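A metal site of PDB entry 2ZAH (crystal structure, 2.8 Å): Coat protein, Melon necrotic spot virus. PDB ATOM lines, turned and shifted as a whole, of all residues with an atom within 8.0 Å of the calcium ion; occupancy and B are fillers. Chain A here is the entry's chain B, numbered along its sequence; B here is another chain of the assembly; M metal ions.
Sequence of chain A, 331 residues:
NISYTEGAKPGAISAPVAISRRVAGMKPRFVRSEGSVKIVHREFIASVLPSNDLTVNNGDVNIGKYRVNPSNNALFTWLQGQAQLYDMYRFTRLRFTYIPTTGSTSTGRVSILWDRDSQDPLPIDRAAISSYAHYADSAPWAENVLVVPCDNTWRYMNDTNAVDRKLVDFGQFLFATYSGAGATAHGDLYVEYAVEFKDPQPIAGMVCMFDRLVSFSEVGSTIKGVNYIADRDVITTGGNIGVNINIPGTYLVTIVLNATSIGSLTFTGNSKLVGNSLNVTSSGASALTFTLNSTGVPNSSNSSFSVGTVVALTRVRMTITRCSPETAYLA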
ATOM      1  N   GLN A  84     -14.929 -18.295  30.288  1.00  0.00           N
ATOM      2  CA  GLN A  84     -16.050 -18.571  29.383  1.00  0.00           C
ATOM      3  C   GLN A  84     -15.686 -18.485  27.906  1.00  0.00           C
ATOM      4  O   GLN A  84     -16.409 -19.028  27.077  1.00  0.00           O
ATOM      5  CB  GLN A  84     -17.244 -17.664  29.713  1.00  0.00           C
ATOM      6  CG  GLN A  84     -16.885 -16.220  29.973  1.00  0.00           C
ATOM      7  CD  GLN A  84     -17.958 -15.254  29.517  1.00  0.00           C
ATOM      8  OE1 GLN A  84     -17.808 -14.036  29.654  1.00  0.00           O
ATOM      9  NE2 GLN A  84     -19.043 -15.780  28.942  1.00  0.00           N
ATOM     10  N   LEU A  85     -14.573 -17.835  27.571  1.00  0.00           N
ATOM     11  CA  LEU A  85     -14.238 -17.582  26.160  1.00  0.00           C
ATOM     12  C   LEU A  85     -13.211 -18.573  25.578  1.00  0.00           C
ATOM     13  O   LEU A  85     -12.841 -18.476  24.405  1.00  0.00           O
ATOM     14  CB  LEU A  85     -13.741 -16.148  25.943  1.00  0.00           C
ATOM     15  CG  LEU A  85     -14.413 -14.885  26.496  1.00  0.00           C
ATOM     16  CD1 LEU A  85     -14.086 -13.701  25.587  1.00  0.00           C
ATOM     17  CD2 LEU A  85     -15.894 -15.034  26.627  1.00  0.00           C
ATOM     18  N   TYR A  86     -12.783 -19.521  26.403  1.00  0.00           N
ATOM     19  CA  TYR A  86     -11.698 -20.416  26.022  1.00  0.00           C
ATOM     20  C   TYR A  86     -11.986 -21.885  26.340  1.00  0.00           C
ATOM     21  O   TYR A  86     -12.803 -22.211  27.199  1.00  0.00           O
ATOM     22  CB  TYR A  86     -10.372 -19.957  26.660  1.00  0.00           C
ATOM     23  CG  TYR A  86      -9.831 -18.663  26.117  1.00  0.00           C
ATOM     24  CD1 TYR A  86     -10.247 -17.437  26.639  1.00  0.00           C
ATOM     25  CD2 TYR A  86      -8.904 -18.640  25.063  1.00  0.00           C
ATOM     26  CE1 TYR A  86      -9.767 -16.251  26.132  1.00  0.00           C
ATOM     27  CE2 TYR A  86      -8.414 -17.452  24.555  1.00  0.00           C
ATOM     28  CZ  TYR A  86      -8.850 -16.259  25.090  1.00  0.00           C
ATOM     29  OH  TYR A  86      -8.360 -15.071  24.582  1.00  0.00           O
ATOM     30  N   ASP A  87     -11.289 -22.783  25.643  1.00  0.00           N
ATOM     31  CA  ASP A  87     -11.539 -24.194  25.757  1.00  0.00           C
ATOM     32  C   ASP A  87     -10.721 -24.938  26.798  1.00  0.00           C
ATOM     33  O   ASP A  87     -11.201 -25.913  27.361  1.00  0.00           O
ATOM     34  CB  ASP A  87     -11.367 -24.873  24.399  1.00  0.00           C
ATOM     35  CG  ASP A  87     -12.705 -25.243  23.762  1.00  0.00           C
ATOM     36  OD1 ASP A  87     -13.568 -25.825  24.488  1.00  0.00           O
ATOM     37  OD2 ASP A  87     -12.910 -24.937  22.552  1.00  0.00           O
ATOM     38  N   MET A  88      -9.488 -24.516  27.032  1.00  0.00           N
ATOM     39  CA  MET A  88      -8.625 -25.271  27.914  1.00  0.00           C
ATOM     40  C   MET A  88      -7.699 -24.382  28.728  1.00  0.00           C
ATOM     41  O   MET A  88      -7.409 -23.256  28.347  1.00  0.00           O
ATOM     42  CB  MET A  88      -7.799 -26.258  27.120  1.00  0.00           C
ATOM     43  CG  MET A  88      -8.593 -27.288  26.368  1.00  0.00           C
ATOM     44  SD  MET A  88      -7.456 -28.507  25.731  1.00  0.00           S
ATOM     45  CE  MET A  88      -7.352 -29.641  27.116  1.00  0.00           C
ATOM     46  N   TYR A 156      -9.612 -29.432  30.197  1.00  0.00           N
ATOM     47  CA  TYR A 156     -10.765 -28.757  29.601  1.00  0.00           C
ATOM     48  C   TYR A 156     -11.467 -27.785  30.521  1.00  0.00           C
ATOM     49  O   TYR A 156     -11.695 -28.068  31.697  1.00  0.00           O
ATOM     50  CB  TYR A 156     -11.764 -29.775  29.049  1.00  0.00           C
ATOM     51  CG  TYR A 156     -11.213 -30.518  27.873  1.00  0.00           C
ATOM     52  CD1 TYR A 156     -11.263 -29.969  26.593  1.00  0.00           C
ATOM     53  CD2 TYR A 156     -10.595 -31.749  28.036  1.00  0.00           C
ATOM     54  CE1 TYR A 156     -10.714 -30.628  25.515  1.00  0.00           C
ATOM     55  CE2 TYR A 156     -10.051 -32.423  26.965  1.00  0.00           C
ATOM     56  CZ  TYR A 156     -10.121 -31.857  25.711  1.00  0.00           C
ATOM     57  OH  TYR A 156      -9.588 -32.525  24.646  1.00  0.00           O
ATOM     58  N   ASP A 199      -7.876 -22.167  23.689  1.00  0.00           N
ATOM     59  CA  ASP A 199      -8.602 -21.878  22.432  1.00  0.00           C
ATOM     60  C   ASP A 199      -9.814 -20.978  22.555  1.00  0.00           C
ATOM     61  O   ASP A 199     -10.768 -21.328  23.228  1.00  0.00           O
ATOM     62  CB  ASP A 199      -8.998 -23.165  21.715  1.00  0.00           C
ATOM     63  CG  ASP A 199      -7.859 -23.732  20.862  1.00  0.00           C
ATOM     64  OD1 ASP A 199      -7.800 -24.967  20.753  1.00  0.00           O
ATOM     65  OD2 ASP A 199      -7.042 -22.955  20.314  1.00  0.00           O
ATOM     66  N   PRO A 200      -9.793 -19.809  21.889  1.00  0.00           N
ATOM     67  CA  PRO A 200     -11.025 -19.019  21.827  1.00  0.00           C
ATOM     68  C   PRO A 200     -12.213 -19.836  21.318  1.00  0.00           C
ATOM     69  O   PRO A 200     -12.099 -20.597  20.355  1.00  0.00           O
ATOM     70  CB  PRO A 200     -10.663 -17.907  20.848  1.00  0.00           C
ATOM     71  CG  PRO A 200      -9.207 -17.776  20.937  1.00  0.00           C
ATOM     72  CD  PRO A 200      -8.678 -19.161  21.194  1.00  0.00           C
ATOM     73  N   GLN A 201     -13.339 -19.679  21.979  1.00  0.00           N
ATOM     74  CA  GLN A 201     -14.556 -20.387  21.625  1.00  0.00           C
ATOM     75  C   GLN A 201     -15.759 -19.438  21.700  1.00  0.00           C
ATOM     76  O   GLN A 201     -15.605 -18.328  22.189  1.00  0.00           O
ATOM     77  CB  GLN A 201     -14.747 -21.580  22.567  1.00  0.00           C
ATOM     78  CG  GLN A 201     -14.928 -21.197  24.027  1.00  0.00           C
ATOM     79  CD  GLN A 201     -15.457 -22.340  24.871  1.00  0.00           C
ATOM     80  OE1 GLN A 201     -15.135 -23.511  24.626  1.00  0.00           O
ATOM     81  NE2 GLN A 201     -16.272 -22.008  25.887  1.00  0.00           N
ATOM     82  N   PRO A 202     -16.937 -19.870  21.201  1.00  0.00           N
ATOM     83  CA  PRO A 202     -18.183 -19.174  21.526  1.00  0.00           C
ATOM     84  C   PRO A 202     -18.311 -19.055  23.026  1.00  0.00           C
ATOM     85  O   PRO A 202     -17.993 -20.023  23.750  1.00  0.00           O
ATOM     86  CB  PRO A 202     -19.256 -20.119  21.010  1.00  0.00           C
ATOM     87  CG  PRO A 202     -18.612 -20.889  19.952  1.00  0.00           C
ATOM     88  CD  PRO A 202     -17.174 -21.015  20.305  1.00  0.00           C
ATOM     89  N   ILE A 203     -18.760 -17.900  23.501  1.00  0.00           N
ATOM     90  CA  ILE A 203     -18.827 -17.658  24.937  1.00  0.00           C
ATOM     91  C   ILE A 203     -19.745 -18.646  25.659  1.00  0.00           C
ATOM     92  O   ILE A 203     -20.821 -18.983  25.161  1.00  0.00           O
ATOM     93  CB  ILE A 203     -19.270 -16.230  25.265  1.00  0.00           C
ATOM     94  CG1 ILE A 203     -20.722 -16.022  24.841  1.00  0.00           C
ATOM     95  CG2 ILE A 203     -18.361 -15.218  24.581  1.00  0.00           C
ATOM     96  CD1 ILE A 203     -21.417 -15.028  25.723  1.00  0.00           C
ATOM     97  N   TRP B 114     -13.781 -26.356  13.936  1.00  0.00           N
ATOM     98  CA  TRP B 114     -13.310 -27.353  14.862  1.00  0.00           C
ATOM     99  C   TRP B 114     -13.321 -26.830  16.301  1.00  0.00           C
ATOM    100  O   TRP B 114     -12.890 -25.709  16.567  1.00  0.00           O
ATOM    101  CB  TRP B 114     -11.930 -27.827  14.439  1.00  0.00           C
ATOM    102  CG  TRP B 114     -11.321 -28.876  15.307  1.00  0.00           C
ATOM    103  CD1 TRP B 114     -11.549 -30.216  15.252  1.00  0.00           C
ATOM    104  CD2 TRP B 114     -10.364 -28.672  16.346  1.00  0.00           C
ATOM    105  NE1 TRP B 114     -10.793 -30.866  16.208  1.00  0.00           N
ATOM    106  CE2 TRP B 114     -10.051 -29.940  16.880  1.00  0.00           C
ATOM    107  CE3 TRP B 114      -9.738 -27.534  16.870  1.00  0.00           C
ATOM    108  CZ2 TRP B 114      -9.136 -30.111  17.924  1.00  0.00           C
ATOM    109  CZ3 TRP B 114      -8.846 -27.697  17.914  1.00  0.00           C
ATOM    110  CH2 TRP B 114      -8.545 -28.976  18.423  1.00  0.00           C
ATOM    111  N   ASP B 115     -13.839 -27.623  17.219  1.00  0.00           N
ATOM    112  CA  ASP B 115     -13.943 -27.265  18.619  1.00  0.00           C
ATOM    113  C   ASP B 115     -13.075 -28.281  19.349  1.00  0.00           C
ATOM    114  O   ASP B 115     -13.280 -29.483  19.168  1.00  0.00           O
ATOM    115  CB  ASP B 115     -15.386 -27.437  19.061  1.00  0.00           C
ATOM    116  CG  ASP B 115     -15.640 -26.989  20.508  1.00  0.00           C
ATOM    117  OD1 ASP B 115     -14.731 -27.147  21.375  1.00  0.00           O
ATOM    118  OD2 ASP B 115     -16.750 -26.484  20.800  1.00  0.00           O
ATOM    119  N   ARG B 116     -12.138 -27.804  20.169  1.00  0.00           N
ATOM    120  CA  ARG B 116     -11.220 -28.715  20.865  1.00  0.00           C
ATOM    121  C   ARG B 116     -11.963 -29.680  21.807  1.00  0.00           C
ATOM    122  O   ARG B 116     -11.489 -30.775  22.105  1.00  0.00           O
ATOM    123  CB  ARG B 116     -10.166 -27.917  21.628  1.00  0.00           C
ATOM    124  CG  ARG B 116      -8.889 -28.700  21.969  1.00  0.00           C
ATOM    125  CD  ARG B 116      -7.721 -27.736  22.197  1.00  0.00           C
ATOM    126  NE  ARG B 116      -6.474 -28.211  21.585  1.00  0.00           N
ATOM    127  CZ  ARG B 116      -5.786 -27.564  20.645  1.00  0.00           C
ATOM    128  NH1 ARG B 116      -6.197 -26.401  20.174  1.00  0.00           N
ATOM    129  NH2 ARG B 116      -4.661 -28.077  20.159  1.00  0.00           N
ATOM    130  N   ASP B 117     -13.130 -29.260  22.285  1.00  0.00           N
ATOM    131  CA  ASP B 117     -13.898 -30.038  23.233  1.00  0.00           C
ATOM    132  C   ASP B 117     -15.027 -30.716  22.460  1.00  0.00           C
ATOM    133  O   ASP B 117     -15.960 -30.051  22.008  1.00  0.00           O
ATOM    134  CB  ASP B 117     -14.429 -29.092  24.293  1.00  0.00           C
ATOM    135  CG  ASP B 117     -15.027 -29.812  25.481  1.00  0.00           C
ATOM    136  OD1 ASP B 117     -15.737 -30.816  25.282  1.00  0.00           O
ATOM    137  OD2 ASP B 117     -14.815 -29.326  26.621  1.00  0.00           O
ATOM    138  N   SER B 118     -14.953 -32.034  22.317  1.00  0.00           N
ATOM    139  CA  SER B 118     -15.937 -32.792  21.539  1.00  0.00           C
ATOM    140  C   SER B 118     -17.264 -32.971  22.241  1.00  0.00           C
ATOM    141  O   SER B 118     -18.162 -33.652  21.727  1.00  0.00           O
ATOM    142  CB  SER B 118     -15.376 -34.181  21.169  1.00  0.00           C
ATOM    143  OG  SER B 118     -15.367 -35.085  22.267  1.00  0.00           O
ATOM    144  N   GLN B 119     -17.404 -32.389  23.426  1.00  0.00           N
ATOM    145  CA  GLN B 119     -18.651 -32.477  24.170  1.00  0.00           C
ATOM    146  C   GLN B 119     -19.358 -31.136  24.332  1.00  0.00           C
ATOM    147  O   GLN B 119     -20.461 -31.089  24.863  1.00  0.00           O
ATOM    148  CB  GLN B 119     -18.420 -33.150  25.517  1.00  0.00           C
ATOM    149  CG  GLN B 119     -18.268 -34.653  25.421  1.00  0.00           C
ATOM    150  CD  GLN B 119     -17.975 -35.333  26.756  1.00  0.00           C
ATOM    151  OE1 GLN B 119     -16.925 -35.130  27.370  1.00  0.00           O
ATOM    152  NE2 GLN B 119     -18.891 -36.186  27.183  1.00  0.00           N
ATOM    153  N   ASP B 120     -18.717 -30.059  23.860  1.00  0.00           N
ATOM    154  CA  ASP B 120     -19.312 -28.724  23.786  1.00  0.00           C
ATOM    155  C   ASP B 120     -20.573 -28.709  22.917  1.00  0.00           C
ATOM    156  O   ASP B 120     -20.628 -29.362  21.877  1.00  0.00           O
ATOM    157  CB  ASP B 120     -18.333 -27.721  23.180  1.00  0.00           C
ATOM    158  CG  ASP B 120     -17.468 -27.029  24.220  1.00  0.00           C
ATOM    159  OD1 ASP B 120     -16.633 -26.187  23.790  1.00  0.00           O
ATOM    160  OD2 ASP B 120     -17.593 -27.302  25.448  1.00  0.00           O
ATOM    161  N   PRO B 121     -21.599 -27.962  23.358  1.00  0.00           N
ATOM    162  CA  PRO B 121     -22.882 -27.832  22.633  1.00  0.00           C
ATOM    163  C   PRO B 121     -22.710 -27.256  21.235  1.00  0.00           C
ATOM    164  O   PRO B 121     -21.740 -26.557  20.982  1.00  0.00           O
ATOM    165  CB  PRO B 121     -23.669 -26.856  23.501  1.00  0.00           C
ATOM    166  CG  PRO B 121     -23.080 -27.040  24.888  1.00  0.00           C
ATOM    167  CD  PRO B 121     -21.623 -27.197  24.617  1.00  0.00           C
ATOM    168  N   SER B 131     -16.795 -17.475  15.890  1.00  0.00           N
ATOM    169  CA  SER B 131     -15.935 -17.226  17.029  1.00  0.00           C
ATOM    170  C   SER B 131     -15.046 -18.383  17.430  1.00  0.00           C
ATOM    171  O   SER B 131     -14.256 -18.236  18.357  1.00  0.00           O
ATOM    172  CB  SER B 131     -16.772 -16.817  18.241  1.00  0.00           C
ATOM    173  OG  SER B 131     -16.856 -15.417  18.334  1.00  0.00           O
ATOM    174  N   TYR B 132     -15.209 -19.537  16.784  1.00  0.00           N
ATOM    175  CA  TYR B 132     -14.286 -20.647  16.999  1.00  0.00           C
ATOM    176  C   TYR B 132     -12.908 -20.195  16.528  1.00  0.00           C
ATOM    177  O   TYR B 132     -12.803 -19.496  15.525  1.00  0.00           O
ATOM    178  CB  TYR B 132     -14.745 -21.869  16.207  1.00  0.00           C
ATOM    179  CG  TYR B 132     -15.979 -22.528  16.762  1.00  0.00           C
ATOM    180  CD1 TYR B 132     -15.855 -23.587  17.667  1.00  0.00           C
ATOM    181  CD2 TYR B 132     -17.253 -22.108  16.395  1.00  0.00           C
ATOM    182  CE1 TYR B 132     -16.971 -24.193  18.198  1.00  0.00           C
ATOM    183  CE2 TYR B 132     -18.391 -22.715  16.921  1.00  0.00           C
ATOM    184  CZ  TYR B 132     -18.238 -23.765  17.821  1.00  0.00           C
ATOM    185  OH  TYR B 132     -19.322 -24.401  18.373  1.00  0.00           O
ATOM    186  N   ALA B 133     -11.873 -20.563  17.288  1.00  0.00           N
ATOM    187  CA  ALA B 133     -10.485 -20.227  16.931  1.00  0.00           C
ATOM    188  C   ALA B 133     -10.145 -20.847  15.594  1.00  0.00           C
ATOM    189  O   ALA B 133      -9.492 -20.221  14.771  1.00  0.00           O
ATOM    190  CB  ALA B 133      -9.539 -20.718  17.984  1.00  0.00           C
ATOM    191  N   GLN B 172     -14.008 -31.954  18.031  1.00  0.00           N
ATOM    192  CA  GLN B 172     -15.051 -32.315  17.094  1.00  0.00           C
ATOM    193  C   GLN B 172     -15.061 -31.331  15.930  1.00  0.00           C
ATOM    194  O   GLN B 172     -14.882 -30.117  16.103  1.00  0.00           O
ATOM    195  CB  GLN B 172     -16.415 -32.319  17.777  1.00  0.00           C
ATOM    196  CG  GLN B 172     -16.854 -30.962  18.347  1.00  0.00           C
ATOM    197  CD  GLN B 172     -18.263 -30.984  18.944  1.00  0.00           C
ATOM    198  OE1 GLN B 172     -19.208 -31.515  18.333  1.00  0.00           O
ATOM    199  NE2 GLN B 172     -18.410 -30.408  20.140  1.00  0.00           N
ATOM    200  N   LEU B 174     -17.379 -29.616  12.999  1.00  0.00           N
ATOM    201  CA  LEU B 174     -18.783 -29.283  12.759  1.00  0.00           C
ATOM    202  C   LEU B 174     -18.854 -28.309  11.599  1.00  0.00           C
ATOM    203  O   LEU B 174     -17.889 -27.601  11.329  1.00  0.00           O
ATOM    204  CB  LEU B 174     -19.449 -28.718  14.025  1.00  0.00           C
ATOM    205  CG  LEU B 174     -18.861 -27.474  14.705  1.00  0.00           C
ATOM    206  CD1 LEU B 174     -19.939 -26.713  15.424  1.00  0.00           C
ATOM    207  CD2 LEU B 174     -17.775 -27.841  15.668  1.00  0.00           C
HETATM  208 CA    CA M   1     -15.308 -24.845  22.194  1.00  0.00          CA
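Within 4 Å of the calcium ion: Asp 87, Gln 201, Asp 115 of chain B and Asp 120 of chain B.
O of Asp 199 lies within hydrogen-bond range of N of Asp 87 (2.9 Å). OD1 of Asp 117 of chain B sits at hydrogen-bond distance from N of Asp 120 of chain B, at 3.4 Å. The backbone carbonyl oxygen (O) of Asp 120 of chain B lies within hydrogen-bond range of the side-chain amide nitrogen (NE2) of Gln 172 of chain B (3.0 Å). OD1 of Asp 115 of chain B sits close to N of Asp 117 of chain B (2.8 Å). The backbone carbonyl oxygen of Asp 115 of chain B sits at hydrogen-bond distance from the backbone NH of Gln 172 of chain B (2.8 Å). The backbone NH (N) of Gln 201 sits at hydrogen-bond distance from the backbone carbonyl oxygen (O) of Leu 85, at 2.8 Å. The side-chain amide nitrogen (NE2) of Gln 201 lies within hydrogen-bond range of the backbone carbonyl oxygen (O) of Gln 84, 3.2 Å away.
The side-chain carboxylate (OD2) of Asp 87 binds the calcium ion (2.4 Å). OD1 of Asp 120 of chain B is bound to the calcium ion, 2.5 Å away. OD1 of Asp 115 of chain B is bound to the calcium ion (2.5 Å). OD2 of Asp 115 of chain B binds the calcium ion (2.6 Å). OE1 of Gln 201 binds the calcium ion (2.8 Å). The calcium ion has five donor atoms within binding distance. Slightly farther from the calcium ion lies OD1 of Asp 87 (3.0 Å).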
